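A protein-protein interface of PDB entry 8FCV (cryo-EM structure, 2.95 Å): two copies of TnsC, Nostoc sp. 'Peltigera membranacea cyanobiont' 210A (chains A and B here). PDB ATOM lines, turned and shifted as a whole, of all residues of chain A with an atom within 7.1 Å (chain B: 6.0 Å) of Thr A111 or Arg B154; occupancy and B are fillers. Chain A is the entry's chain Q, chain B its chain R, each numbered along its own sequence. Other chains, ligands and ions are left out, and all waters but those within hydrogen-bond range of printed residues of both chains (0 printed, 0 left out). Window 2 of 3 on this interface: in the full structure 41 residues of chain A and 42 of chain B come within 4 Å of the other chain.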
ATOM      1  N   ILE A  97      14.655  -5.698 -18.046  1.00  0.00           N
ATOM      2  CA  ILE A  97      14.683  -5.804 -16.593  1.00  0.00           C
ATOM      3  C   ILE A  97      13.938  -7.062 -16.179  1.00  0.00           C
ATOM      4  O   ILE A  97      12.802  -7.290 -16.614  1.00  0.00           O
ATOM      5  CB  ILE A  97      14.066  -4.563 -15.926  1.00  0.00           C
ATOM      6  CG1 ILE A  97      14.820  -3.302 -16.348  1.00  0.00           C
ATOM      7  CG2 ILE A  97      14.055  -4.723 -14.411  1.00  0.00           C
ATOM      8  CD1 ILE A  97      14.636  -2.137 -15.407  1.00  0.00           C
ATOM      9  N   ASN A 105       6.818  -7.254 -16.681  1.00  0.00           N
ATOM     10  CA  ASN A 105       6.080  -5.998 -16.646  1.00  0.00           C
ATOM     11  C   ASN A 105       6.392  -5.229 -17.924  1.00  0.00           C
ATOM     12  O   ASN A 105       7.563  -5.006 -18.250  1.00  0.00           O
ATOM     13  CB  ASN A 105       6.454  -5.192 -15.397  1.00  0.00           C
ATOM     14  CG  ASN A 105       5.828  -3.796 -15.361  1.00  0.00           C
ATOM     15  OD1 ASN A 105       5.797  -3.069 -16.353  1.00  0.00           O
ATOM     16  ND2 ASN A 105       5.324  -3.421 -14.190  1.00  0.00           N
ATOM     17  N   TRP A 106       5.345  -4.823 -18.641  1.00  0.00           N
ATOM     18  CA  TRP A 106       5.503  -4.074 -19.879  1.00  0.00           C
ATOM     19  C   TRP A 106       5.384  -2.570 -19.693  1.00  0.00           C
ATOM     20  O   TRP A 106       5.933  -1.815 -20.506  1.00  0.00           O
ATOM     21  CB  TRP A 106       4.477  -4.544 -20.910  1.00  0.00           C
ATOM     22  CG  TRP A 106       4.819  -5.873 -21.474  1.00  0.00           C
ATOM     23  CD1 TRP A 106       4.430  -7.092 -21.005  1.00  0.00           C
ATOM     24  CD2 TRP A 106       5.643  -6.123 -22.614  1.00  0.00           C
ATOM     25  NE1 TRP A 106       4.960  -8.088 -21.789  1.00  0.00           N
ATOM     26  CE2 TRP A 106       5.708  -7.515 -22.784  1.00  0.00           C
ATOM     27  CE3 TRP A 106       6.330  -5.300 -23.510  1.00  0.00           C
ATOM     28  CZ2 TRP A 106       6.434  -8.106 -23.812  1.00  0.00           C
ATOM     29  CZ3 TRP A 106       7.047  -5.887 -24.531  1.00  0.00           C
ATOM     30  CH2 TRP A 106       7.095  -7.276 -24.674  1.00  0.00           C
ATOM     31  N   LYS A 107       4.684  -2.114 -18.653  1.00  0.00           N
ATOM     32  CA  LYS A 107       4.665  -0.688 -18.356  1.00  0.00           C
ATOM     33  C   LYS A 107       6.068  -0.187 -18.046  1.00  0.00           C
ATOM     34  O   LYS A 107       6.469   0.890 -18.507  1.00  0.00           O
ATOM     35  CB  LYS A 107       3.714  -0.410 -17.191  1.00  0.00           C
ATOM     36  CG  LYS A 107       3.292   1.044 -17.054  1.00  0.00           C
ATOM     37  CD  LYS A 107       2.094   1.178 -16.125  1.00  0.00           C
ATOM     38  CE  LYS A 107       1.695   2.631 -15.934  1.00  0.00           C
ATOM     39  NZ  LYS A 107       2.815   3.450 -15.393  1.00  0.00           N
ATOM     40  N   GLU A 108       6.834  -0.966 -17.278  1.00  0.00           N
ATOM     41  CA  GLU A 108       8.223  -0.611 -17.005  1.00  0.00           C
ATOM     42  C   GLU A 108       9.047  -0.580 -18.286  1.00  0.00           C
ATOM     43  O   GLU A 108       9.868   0.322 -18.482  1.00  0.00           O
ATOM     44  CB  GLU A 108       8.831  -1.595 -16.009  1.00  0.00           C
ATOM     45  CG  GLU A 108       8.998  -1.035 -14.611  1.00  0.00           C
ATOM     46  CD  GLU A 108      10.073   0.031 -14.529  1.00  0.00           C
ATOM     47  OE1 GLU A 108       9.754   1.217 -14.755  1.00  0.00           O
ATOM     48  OE2 GLU A 108      11.236  -0.318 -14.240  1.00  0.00           O
ATOM     49  N   TYR A 109       8.845  -1.562 -19.166  1.00  0.00           N
ATOM     50  CA  TYR A 109       9.563  -1.588 -20.436  1.00  0.00           C
ATOM     51  C   TYR A 109       9.287  -0.328 -21.247  1.00  0.00           C
ATOM     52  O   TYR A 109      10.214   0.331 -21.735  1.00  0.00           O
ATOM     53  CB  TYR A 109       9.165  -2.836 -21.223  1.00  0.00           C
ATOM     54  CG  TYR A 109       9.944  -3.056 -22.499  1.00  0.00           C
ATOM     55  CD1 TYR A 109      11.309  -2.823 -22.557  1.00  0.00           C
ATOM     56  CD2 TYR A 109       9.305  -3.493 -23.650  1.00  0.00           C
ATOM     57  CE1 TYR A 109      12.016  -3.025 -23.725  1.00  0.00           C
ATOM     58  CE2 TYR A 109      10.002  -3.697 -24.821  1.00  0.00           C
ATOM     59  CZ  TYR A 109      11.358  -3.461 -24.854  1.00  0.00           C
ATOM     60  OH  TYR A 109      12.054  -3.664 -26.023  1.00  0.00           O
ATOM     61  N   TYR A 110       8.008   0.029 -21.387  1.00  0.00           N
ATOM     62  CA  TYR A 110       7.650   1.199 -22.180  1.00  0.00           C
ATOM     63  C   TYR A 110       8.184   2.483 -21.557  1.00  0.00           C
ATOM     64  O   TYR A 110       8.711   3.351 -22.265  1.00  0.00           O
ATOM     65  CB  TYR A 110       6.135   1.273 -22.356  1.00  0.00           C
ATOM     66  CG  TYR A 110       5.552   0.117 -23.138  1.00  0.00           C
ATOM     67  CD1 TYR A 110       6.324  -0.581 -24.056  1.00  0.00           C
ATOM     68  CD2 TYR A 110       4.231  -0.270 -22.963  1.00  0.00           C
ATOM     69  CE1 TYR A 110       5.797  -1.637 -24.775  1.00  0.00           C
ATOM     70  CE2 TYR A 110       3.696  -1.324 -23.679  1.00  0.00           C
ATOM     71  CZ  TYR A 110       4.484  -2.003 -24.582  1.00  0.00           C
ATOM     72  OH  TYR A 110       3.955  -3.053 -25.297  1.00  0.00           O
ATOM     73  N   THR A 111       8.068   2.627 -20.232  1.00  0.00           N
ATOM     74  CA  THR A 111       8.524   3.867 -19.613  1.00  0.00           C
ATOM     75  C   THR A 111      10.045   3.978 -19.653  1.00  0.00           C
ATOM     76  O   THR A 111      10.583   5.078 -19.807  1.00  0.00           O
ATOM     77  CB  THR A 111       8.000   3.995 -18.180  1.00  0.00           C
ATOM     78  OG1 THR A 111       8.353   5.281 -17.657  1.00  0.00           O
ATOM     79  CG2 THR A 111       8.587   2.931 -17.279  1.00  0.00           C
ATOM     80  N   ARG A 112      10.758   2.854 -19.548  1.00  0.00           N
ATOM     81  CA  ARG A 112      12.212   2.901 -19.665  1.00  0.00           C
ATOM     82  C   ARG A 112      12.637   3.247 -21.084  1.00  0.00           C
ATOM     83  O   ARG A 112      13.586   4.016 -21.286  1.00  0.00           O
ATOM     84  CB  ARG A 112      12.819   1.569 -19.230  1.00  0.00           C
ATOM     85  CG  ARG A 112      14.256   1.677 -18.758  1.00  0.00           C
ATOM     86  CD  ARG A 112      14.538   0.693 -17.639  1.00  0.00           C
ATOM     87  NE  ARG A 112      13.609   0.856 -16.527  1.00  0.00           N
ATOM     88  CZ  ARG A 112      13.953   1.270 -15.315  1.00  0.00           C
ATOM     89  NH1 ARG A 112      15.206   1.575 -15.021  1.00  0.00           N
ATOM     90  NH2 ARG A 112      13.019   1.376 -14.376  1.00  0.00           N
ATOM     91  N   ALA A 113      11.944   2.691 -22.083  1.00  0.00           N
ATOM     92  CA  ALA A 113      12.229   3.063 -23.463  1.00  0.00           C
ATOM     93  C   ALA A 113      11.976   4.548 -23.690  1.00  0.00           C
ATOM     94  O   ALA A 113      12.739   5.215 -24.398  1.00  0.00           O
ATOM     95  CB  ALA A 113      11.389   2.218 -24.419  1.00  0.00           C
ATOM     96  N   LEU A 114      10.908   5.084 -23.093  1.00  0.00           N
ATOM     97  CA  LEU A 114      10.644   6.516 -23.197  1.00  0.00           C
ATOM     98  C   LEU A 114      11.730   7.335 -22.507  1.00  0.00           C
ATOM     99  O   LEU A 114      12.128   8.395 -23.005  1.00  0.00           O
ATOM    100  CB  LEU A 114       9.270   6.840 -22.613  1.00  0.00           C
ATOM    101  CG  LEU A 114       8.076   6.371 -23.444  1.00  0.00           C
ATOM    102  CD1 LEU A 114       6.780   6.942 -22.897  1.00  0.00           C
ATOM    103  CD2 LEU A 114       8.264   6.759 -24.900  1.00  0.00           C
ATOM    104  N   ILE A 115      12.214   6.864 -21.354  1.00  0.00           N
ATOM    105  CA  ILE A 115      13.293   7.558 -20.655  1.00  0.00           C
ATOM    106  C   ILE A 115      14.542   7.605 -21.523  1.00  0.00           C
ATOM    107  O   ILE A 115      15.234   8.629 -21.587  1.00  0.00           O
ATOM    108  CB  ILE A 115      13.574   6.889 -19.296  1.00  0.00           C
ATOM    109  CG1 ILE A 115      12.403   7.103 -18.338  1.00  0.00           C
ATOM    110  CG2 ILE A 115      14.858   7.429 -18.687  1.00  0.00           C
ATOM    111  CD1 ILE A 115      12.645   6.565 -16.951  1.00  0.00           C
ATOM    112  N   THR A 116      14.851   6.499 -22.204  1.00  0.00           N
ATOM    113  CA  THR A 116      16.031   6.468 -23.062  1.00  0.00           C
ATOM    114  C   THR A 116      15.926   7.501 -24.181  1.00  0.00           C
ATOM    115  O   THR A 116      16.910   8.177 -24.505  1.00  0.00           O
ATOM    116  CB  THR A 116      16.225   5.067 -23.639  1.00  0.00           C
ATOM    117  OG1 THR A 116      16.475   4.144 -22.572  1.00  0.00           O
ATOM    118  CG2 THR A 116      17.403   5.044 -24.599  1.00  0.00           C
ATOM    119  N   LEU A 117      14.742   7.647 -24.772  1.00  0.00           N
ATOM    120  CA  LEU A 117      14.521   8.607 -25.847  1.00  0.00           C
ATOM    121  C   LEU A 117      14.367  10.042 -25.352  1.00  0.00           C
ATOM    122  O   LEU A 117      14.009  10.913 -26.152  1.00  0.00           O
ATOM    123  CB  LEU A 117      13.285   8.212 -26.660  1.00  0.00           C
ATOM    124  CG  LEU A 117      13.237   6.771 -27.167  1.00  0.00           C
ATOM    125  CD1 LEU A 117      11.901   6.476 -27.826  1.00  0.00           C
ATOM    126  CD2 LEU A 117      14.377   6.517 -28.130  1.00  0.00           C
ATOM    127  N   GLU A 119      12.086  11.381 -23.546  1.00  0.00           N
ATOM    128  CA  GLU A 119      10.711  11.840 -23.679  1.00  0.00           C
ATOM    129  C   GLU A 119      10.374  12.797 -22.540  1.00  0.00           C
ATOM    130  O   GLU A 119      10.636  12.479 -21.372  1.00  0.00           O
ATOM    131  CB  GLU A 119       9.759  10.644 -23.668  1.00  0.00           C
ATOM    132  CG  GLU A 119       8.276  10.986 -23.650  1.00  0.00           C
ATOM    133  CD  GLU A 119       7.860  11.883 -24.798  1.00  0.00           C
ATOM    134  OE1 GLU A 119       8.159  11.537 -25.961  1.00  0.00           O
ATOM    135  OE2 GLU A 119       7.215  12.920 -24.543  1.00  0.00           O
ATOM    136  N   ILE A 122       7.023  12.063 -19.019  1.00  0.00           N
ATOM    137  CA  ILE A 122       6.671  10.655 -19.184  1.00  0.00           C
ATOM    138  C   ILE A 122       5.589  10.250 -18.190  1.00  0.00           C
ATOM    139  O   ILE A 122       4.608   9.589 -18.549  1.00  0.00           O
ATOM    140  CB  ILE A 122       7.921   9.769 -19.044  1.00  0.00           C
ATOM    141  CG1 ILE A 122       9.019  10.264 -19.983  1.00  0.00           C
ATOM    142  CG2 ILE A 122       7.583   8.317 -19.337  1.00  0.00           C
ATOM    143  CD1 ILE A 122      10.369   9.658 -19.717  1.00  0.00           C
ATOM    144  N   ASP A 123       5.756  10.637 -16.924  1.00  0.00           N
ATOM    145  CA  ASP A 123       4.827  10.194 -15.888  1.00  0.00           C
ATOM    146  C   ASP A 123       3.423  10.739 -16.120  1.00  0.00           C
ATOM    147  O   ASP A 123       2.436  10.016 -15.942  1.00  0.00           O
ATOM    148  CB  ASP A 123       5.341  10.610 -14.510  1.00  0.00           C
ATOM    149  CG  ASP A 123       4.577   9.948 -13.379  1.00  0.00           C
ATOM    150  OD1 ASP A 123       3.903   8.926 -13.631  1.00  0.00           O
ATOM    151  OD2 ASP A 123       4.649  10.447 -12.237  1.00  0.00           O
ATOM    152  N   LEU A 152       1.152   4.685 -22.716  1.00  0.00           N
ATOM    153  CA  LEU A 152       2.603   4.551 -22.793  1.00  0.00           C
ATOM    154  C   LEU A 152       3.023   3.873 -24.090  1.00  0.00           C
ATOM    155  O   LEU A 152       4.008   4.274 -24.721  1.00  0.00           O
ATOM    156  CB  LEU A 152       3.114   3.767 -21.585  1.00  0.00           C
ATOM    157  CG  LEU A 152       4.383   4.279 -20.905  1.00  0.00           C
ATOM    158  CD1 LEU A 152       4.234   5.744 -20.533  1.00  0.00           C
ATOM    159  CD2 LEU A 152       4.695   3.440 -19.679  1.00  0.00           C
ATOM    160  N   LEU A 156       5.341   5.497 -26.997  1.00  0.00           N
ATOM    161  CA  LEU A 156       6.548   4.854 -27.508  1.00  0.00           C
ATOM    162  C   LEU A 156       6.487   4.689 -29.020  1.00  0.00           C
ATOM    163  O   LEU A 156       7.485   4.904 -29.717  1.00  0.00           O
ATOM    164  CB  LEU A 156       6.752   3.502 -26.828  1.00  0.00           C
ATOM    165  CG  LEU A 156       8.029   2.754 -27.213  1.00  0.00           C
ATOM    166  CD1 LEU A 156       9.247   3.636 -26.995  1.00  0.00           C
ATOM    167  CD2 LEU A 156       8.151   1.464 -26.423  1.00  0.00           C
ATOM    168  N   VAL B 130      10.551   9.807 -10.119  1.00  0.00           N
ATOM    169  CA  VAL B 130       9.223   9.484  -9.599  1.00  0.00           C
ATOM    170  C   VAL B 130       8.769  10.561  -8.620  1.00  0.00           C
ATOM    171  O   VAL B 130       9.560  11.073  -7.820  1.00  0.00           O
ATOM    172  CB  VAL B 130       9.185   8.084  -8.951  1.00  0.00           C
ATOM    173  CG1 VAL B 130       7.756   7.687  -8.621  1.00  0.00           C
ATOM    174  CG2 VAL B 130       9.826   7.055  -9.869  1.00  0.00           C
ATOM    175  N   ALA B 149       5.839  -0.392  -6.780  1.00  0.00           N
ATOM    176  CA  ALA B 149       7.173  -0.920  -6.503  1.00  0.00           C
ATOM    177  C   ALA B 149       8.174  -0.670  -7.628  1.00  0.00           C
ATOM    178  O   ALA B 149       9.314  -0.278  -7.325  1.00  0.00           O
ATOM    179  CB  ALA B 149       7.072  -2.410  -6.162  1.00  0.00           C
ATOM    180  N   PRO B 150       7.856  -0.898  -8.911  1.00  0.00           N
ATOM    181  CA  PRO B 150       8.869  -0.649  -9.955  1.00  0.00           C
ATOM    182  C   PRO B 150       9.359   0.792 -10.026  1.00  0.00           C
ATOM    183  O   PRO B 150      10.536   1.021 -10.329  1.00  0.00           O
ATOM    184  CB  PRO B 150       8.143  -1.067 -11.239  1.00  0.00           C
ATOM    185  CG  PRO B 150       7.141  -2.059 -10.791  1.00  0.00           C
ATOM    186  CD  PRO B 150       6.655  -1.539  -9.479  1.00  0.00           C
ATOM    187  N   ALA B 151       8.490   1.772  -9.768  1.00  0.00           N
ATOM    188  CA  ALA B 151       8.939   3.161  -9.752  1.00  0.00           C
ATOM    189  C   ALA B 151       9.918   3.408  -8.611  1.00  0.00           C
ATOM    190  O   ALA B 151      10.923   4.115  -8.776  1.00  0.00           O
ATOM    191  CB  ALA B 151       7.737   4.098  -9.645  1.00  0.00           C
ATOM    192  N   LEU B 152       9.638   2.829  -7.443  1.00  0.00           N
ATOM    193  CA  LEU B 152      10.575   2.891  -6.330  1.00  0.00           C
ATOM    194  C   LEU B 152      11.896   2.229  -6.696  1.00  0.00           C
ATOM    195  O   LEU B 152      12.972   2.719  -6.332  1.00  0.00           O
ATOM    196  CB  LEU B 152       9.948   2.219  -5.110  1.00  0.00           C
ATOM    197  CG  LEU B 152      10.790   1.968  -3.863  1.00  0.00           C
ATOM    198  CD1 LEU B 152      11.464   3.245  -3.393  1.00  0.00           C
ATOM    199  CD2 LEU B 152       9.909   1.378  -2.777  1.00  0.00           C
ATOM    200  N   ARG B 153      11.830   1.115  -7.428  1.00  0.00           N
ATOM    201  CA  ARG B 153      13.040   0.451  -7.895  1.00  0.00           C
ATOM    202  C   ARG B 153      13.852   1.362  -8.805  1.00  0.00           C
ATOM    203  O   ARG B 153      15.074   1.454  -8.668  1.00  0.00           O
ATOM    204  CB  ARG B 153      12.675  -0.841  -8.622  1.00  0.00           C
ATOM    205  CG  ARG B 153      13.829  -1.494  -9.359  1.00  0.00           C
ATOM    206  CD  ARG B 153      13.440  -2.877  -9.858  1.00  0.00           C
ATOM    207  NE  ARG B 153      14.588  -3.671 -10.284  1.00  0.00           N
ATOM    208  CZ  ARG B 153      15.326  -3.415 -11.356  1.00  0.00           C
ATOM    209  NH1 ARG B 153      15.069  -2.384 -12.144  1.00  0.00           N
ATOM    210  NH2 ARG B 153      16.343  -4.220 -11.649  1.00  0.00           N
ATOM    211  N   ARG B 154      13.186   2.039  -9.740  1.00  0.00           N
ATOM    212  CA  ARG B 154      13.882   2.948 -10.647  1.00  0.00           C
ATOM    213  C   ARG B 154      14.518   4.106  -9.887  1.00  0.00           C
ATOM    214  O   ARG B 154      15.634   4.540 -10.209  1.00  0.00           O
ATOM    215  CB  ARG B 154      12.915   3.469 -11.708  1.00  0.00           C
ATOM    216  CG  ARG B 154      13.566   4.318 -12.782  1.00  0.00           C
ATOM    217  CD  ARG B 154      12.550   4.800 -13.805  1.00  0.00           C
ATOM    218  NE  ARG B 154      11.400   3.909 -13.906  1.00  0.00           N
ATOM    219  CZ  ARG B 154      10.156   4.253 -13.605  1.00  0.00           C
ATOM    220  NH1 ARG B 154       9.861   5.470 -13.178  1.00  0.00           N
ATOM    221  NH2 ARG B 154       9.185   3.354 -13.733  1.00  0.00           N
ATOM    222  N   ALA B 155      13.812   4.631  -8.884  1.00  0.00           N
ATOM    223  CA  ALA B 155      14.397   5.670  -8.043  1.00  0.00           C
ATOM    224  C   ALA B 155      15.635   5.154  -7.321  1.00  0.00           C
ATOM    225  O   ALA B 155      16.636   5.871  -7.195  1.00  0.00           O
ATOM    226  CB  ALA B 155      13.363   6.184  -7.043  1.00  0.00           C
ATOM    227  N   LEU B 156      15.581   3.911  -6.838  1.00  0.00           N
ATOM    228  CA  LEU B 156      16.752   3.305  -6.215  1.00  0.00           C
ATOM    229  C   LEU B 156      17.900   3.178  -7.211  1.00  0.00           C
ATOM    230  O   LEU B 156      19.064   3.382  -6.854  1.00  0.00           O
ATOM    231  CB  LEU B 156      16.393   1.940  -5.633  1.00  0.00           C
ATOM    232  CG  LEU B 156      17.541   1.173  -4.976  1.00  0.00           C
ATOM    233  CD1 LEU B 156      18.080   1.943  -3.780  1.00  0.00           C
ATOM    234  CD2 LEU B 156      17.096  -0.219  -4.565  1.00  0.00           C
ATOM    235  N   GLU B 157      17.589   2.822  -8.459  1.00  0.00           N
ATOM    236  CA  GLU B 157      18.618   2.750  -9.495  1.00  0.00           C
ATOM    237  C   GLU B 157      19.294   4.099  -9.689  1.00  0.00           C
ATOM    238  O   GLU B 157      20.526   4.187  -9.762  1.00  0.00           O
ATOM    239  CB  GLU B 157      18.010   2.286 -10.817  1.00  0.00           C
ATOM    240  CG  GLU B 157      17.167   1.040 -10.720  1.00  0.00           C
ATOM    241  CD  GLU B 157      17.665  -0.081 -11.593  1.00  0.00           C
ATOM    242  OE1 GLU B 157      18.848  -0.463 -11.474  1.00  0.00           O
ATOM    243  OE2 GLU B 157      16.859  -0.581 -12.403  1.00  0.00           O
ATOM    244  N   ASN B 158      18.494   5.163  -9.795  1.00  0.00           N
ATOM    245  CA  ASN B 158      19.054   6.499  -9.975  1.00  0.00           C
ATOM    246  C   ASN B 158      19.910   6.897  -8.778  1.00  0.00           C
ATOM    247  O   ASN B 158      21.007   7.451  -8.935  1.00  0.00           O
ATOM    248  CB  ASN B 158      17.934   7.512 -10.205  1.00  0.00           C
ATOM    249  CG  ASN B 158      17.074   7.164 -11.401  1.00  0.00           C
ATOM    250  OD1 ASN B 158      17.581   6.756 -12.446  1.00  0.00           O
ATOM    251  ND2 ASN B 158      15.765   7.323 -11.256  1.00  0.00           N
ATOM    252  N   ALA B 159      19.425   6.611  -7.568  1.00  0.00           N
ATOM    253  CA  ALA B 159      20.189   6.938  -6.370  1.00  0.00           C
ATOM    254  C   ALA B 159      21.509   6.180  -6.335  1.00  0.00           C
ATOM    255  O   ALA B 159      22.547   6.744  -5.972  1.00  0.00           O
ATOM    256  CB  ALA B 159      19.362   6.631  -5.123  1.00  0.00           C
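Thr A111 touches just one residue of chain B: Arg B154. Arg B154 touches four residues of chain A. Of the printed residues of chain B, Arg A112 touches Arg B154 (3.0 Å) and Glu B157 (3.8 Å). Printed residues of chain B within 4 Å of Ile A97: Arg B153 (3.3 Å). Of the printed residues of chain B, Ile A115 touches Arg B154. Val B130 touches none of the printed residues of chain A. The nearest residue of chain A that does not touch Arg B154 is Lys A107 (6.0 Å). The nearest printed residue of chain B that does not touch Glu A108 is Arg B153 (4.8 Å).
Printed residues of chain B that touch a printed residue of chain A: Pro B150, Arg B153, Arg B154 and Glu B157. Along chain B the printed residues that touch a printed residue of chain A span positions 150 to 157. Along chain A the printed residues that touch a printed residue of chain B span positions 97 to 115. Among the printed residues, Asp or Glu carboxylates within 4 Å of a Lys or Arg side-chain nitrogen of the other chain: Glu A108 with Arg B154 (2.4 Å) and Arg A112 with Glu B157 (3.8 Å).
Among the printed residues, merely in contact across the chains: Ile A97 with Arg B153 (3.3 Å), Glu A108 with Pro B150 (3.5 Å), Thr A111 with Arg B154 (3.6 Å) and Ile A115 with Arg B154 (3.6 Å).
The guanidinium group (NH1) of Arg A112 is in salt-bridge range of the side-chain carboxylate (OE2) of Glu B157 (3.8 Å). NH2 of Arg B154 is in salt-bridge range of OE1 of Glu A108 (2.4 Å). The guanidinium group (NH2) of Arg A112 sits close to the guanidinium group (NE) of Arg B154.
2 positions are printed for both chains. Of the 7 pairs that touch across the chains among the printed residues, none has its exchanged pair printed and touching as well.
ND2 of Asn B158 lies within hydrogen-bond range of O of Arg B154 (3.0 Å). The side-chain amide oxygen (OD1) of Asn A105 is in hydrogen-bond range of the backbone NH (N) of Glu A108. The backbone carbonyl oxygen of Arg A112 sits at hydrogen-bond distance from the side-chain hydroxyl of Thr A116 (3.2 Å). NH1 of Arg B153 is in salt-bridge range of OE2 of Glu B157 (2.6 Å). OE2 of Glu A108 is in salt-bridge range of NH2 of Arg A112, at 2.5 Å.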
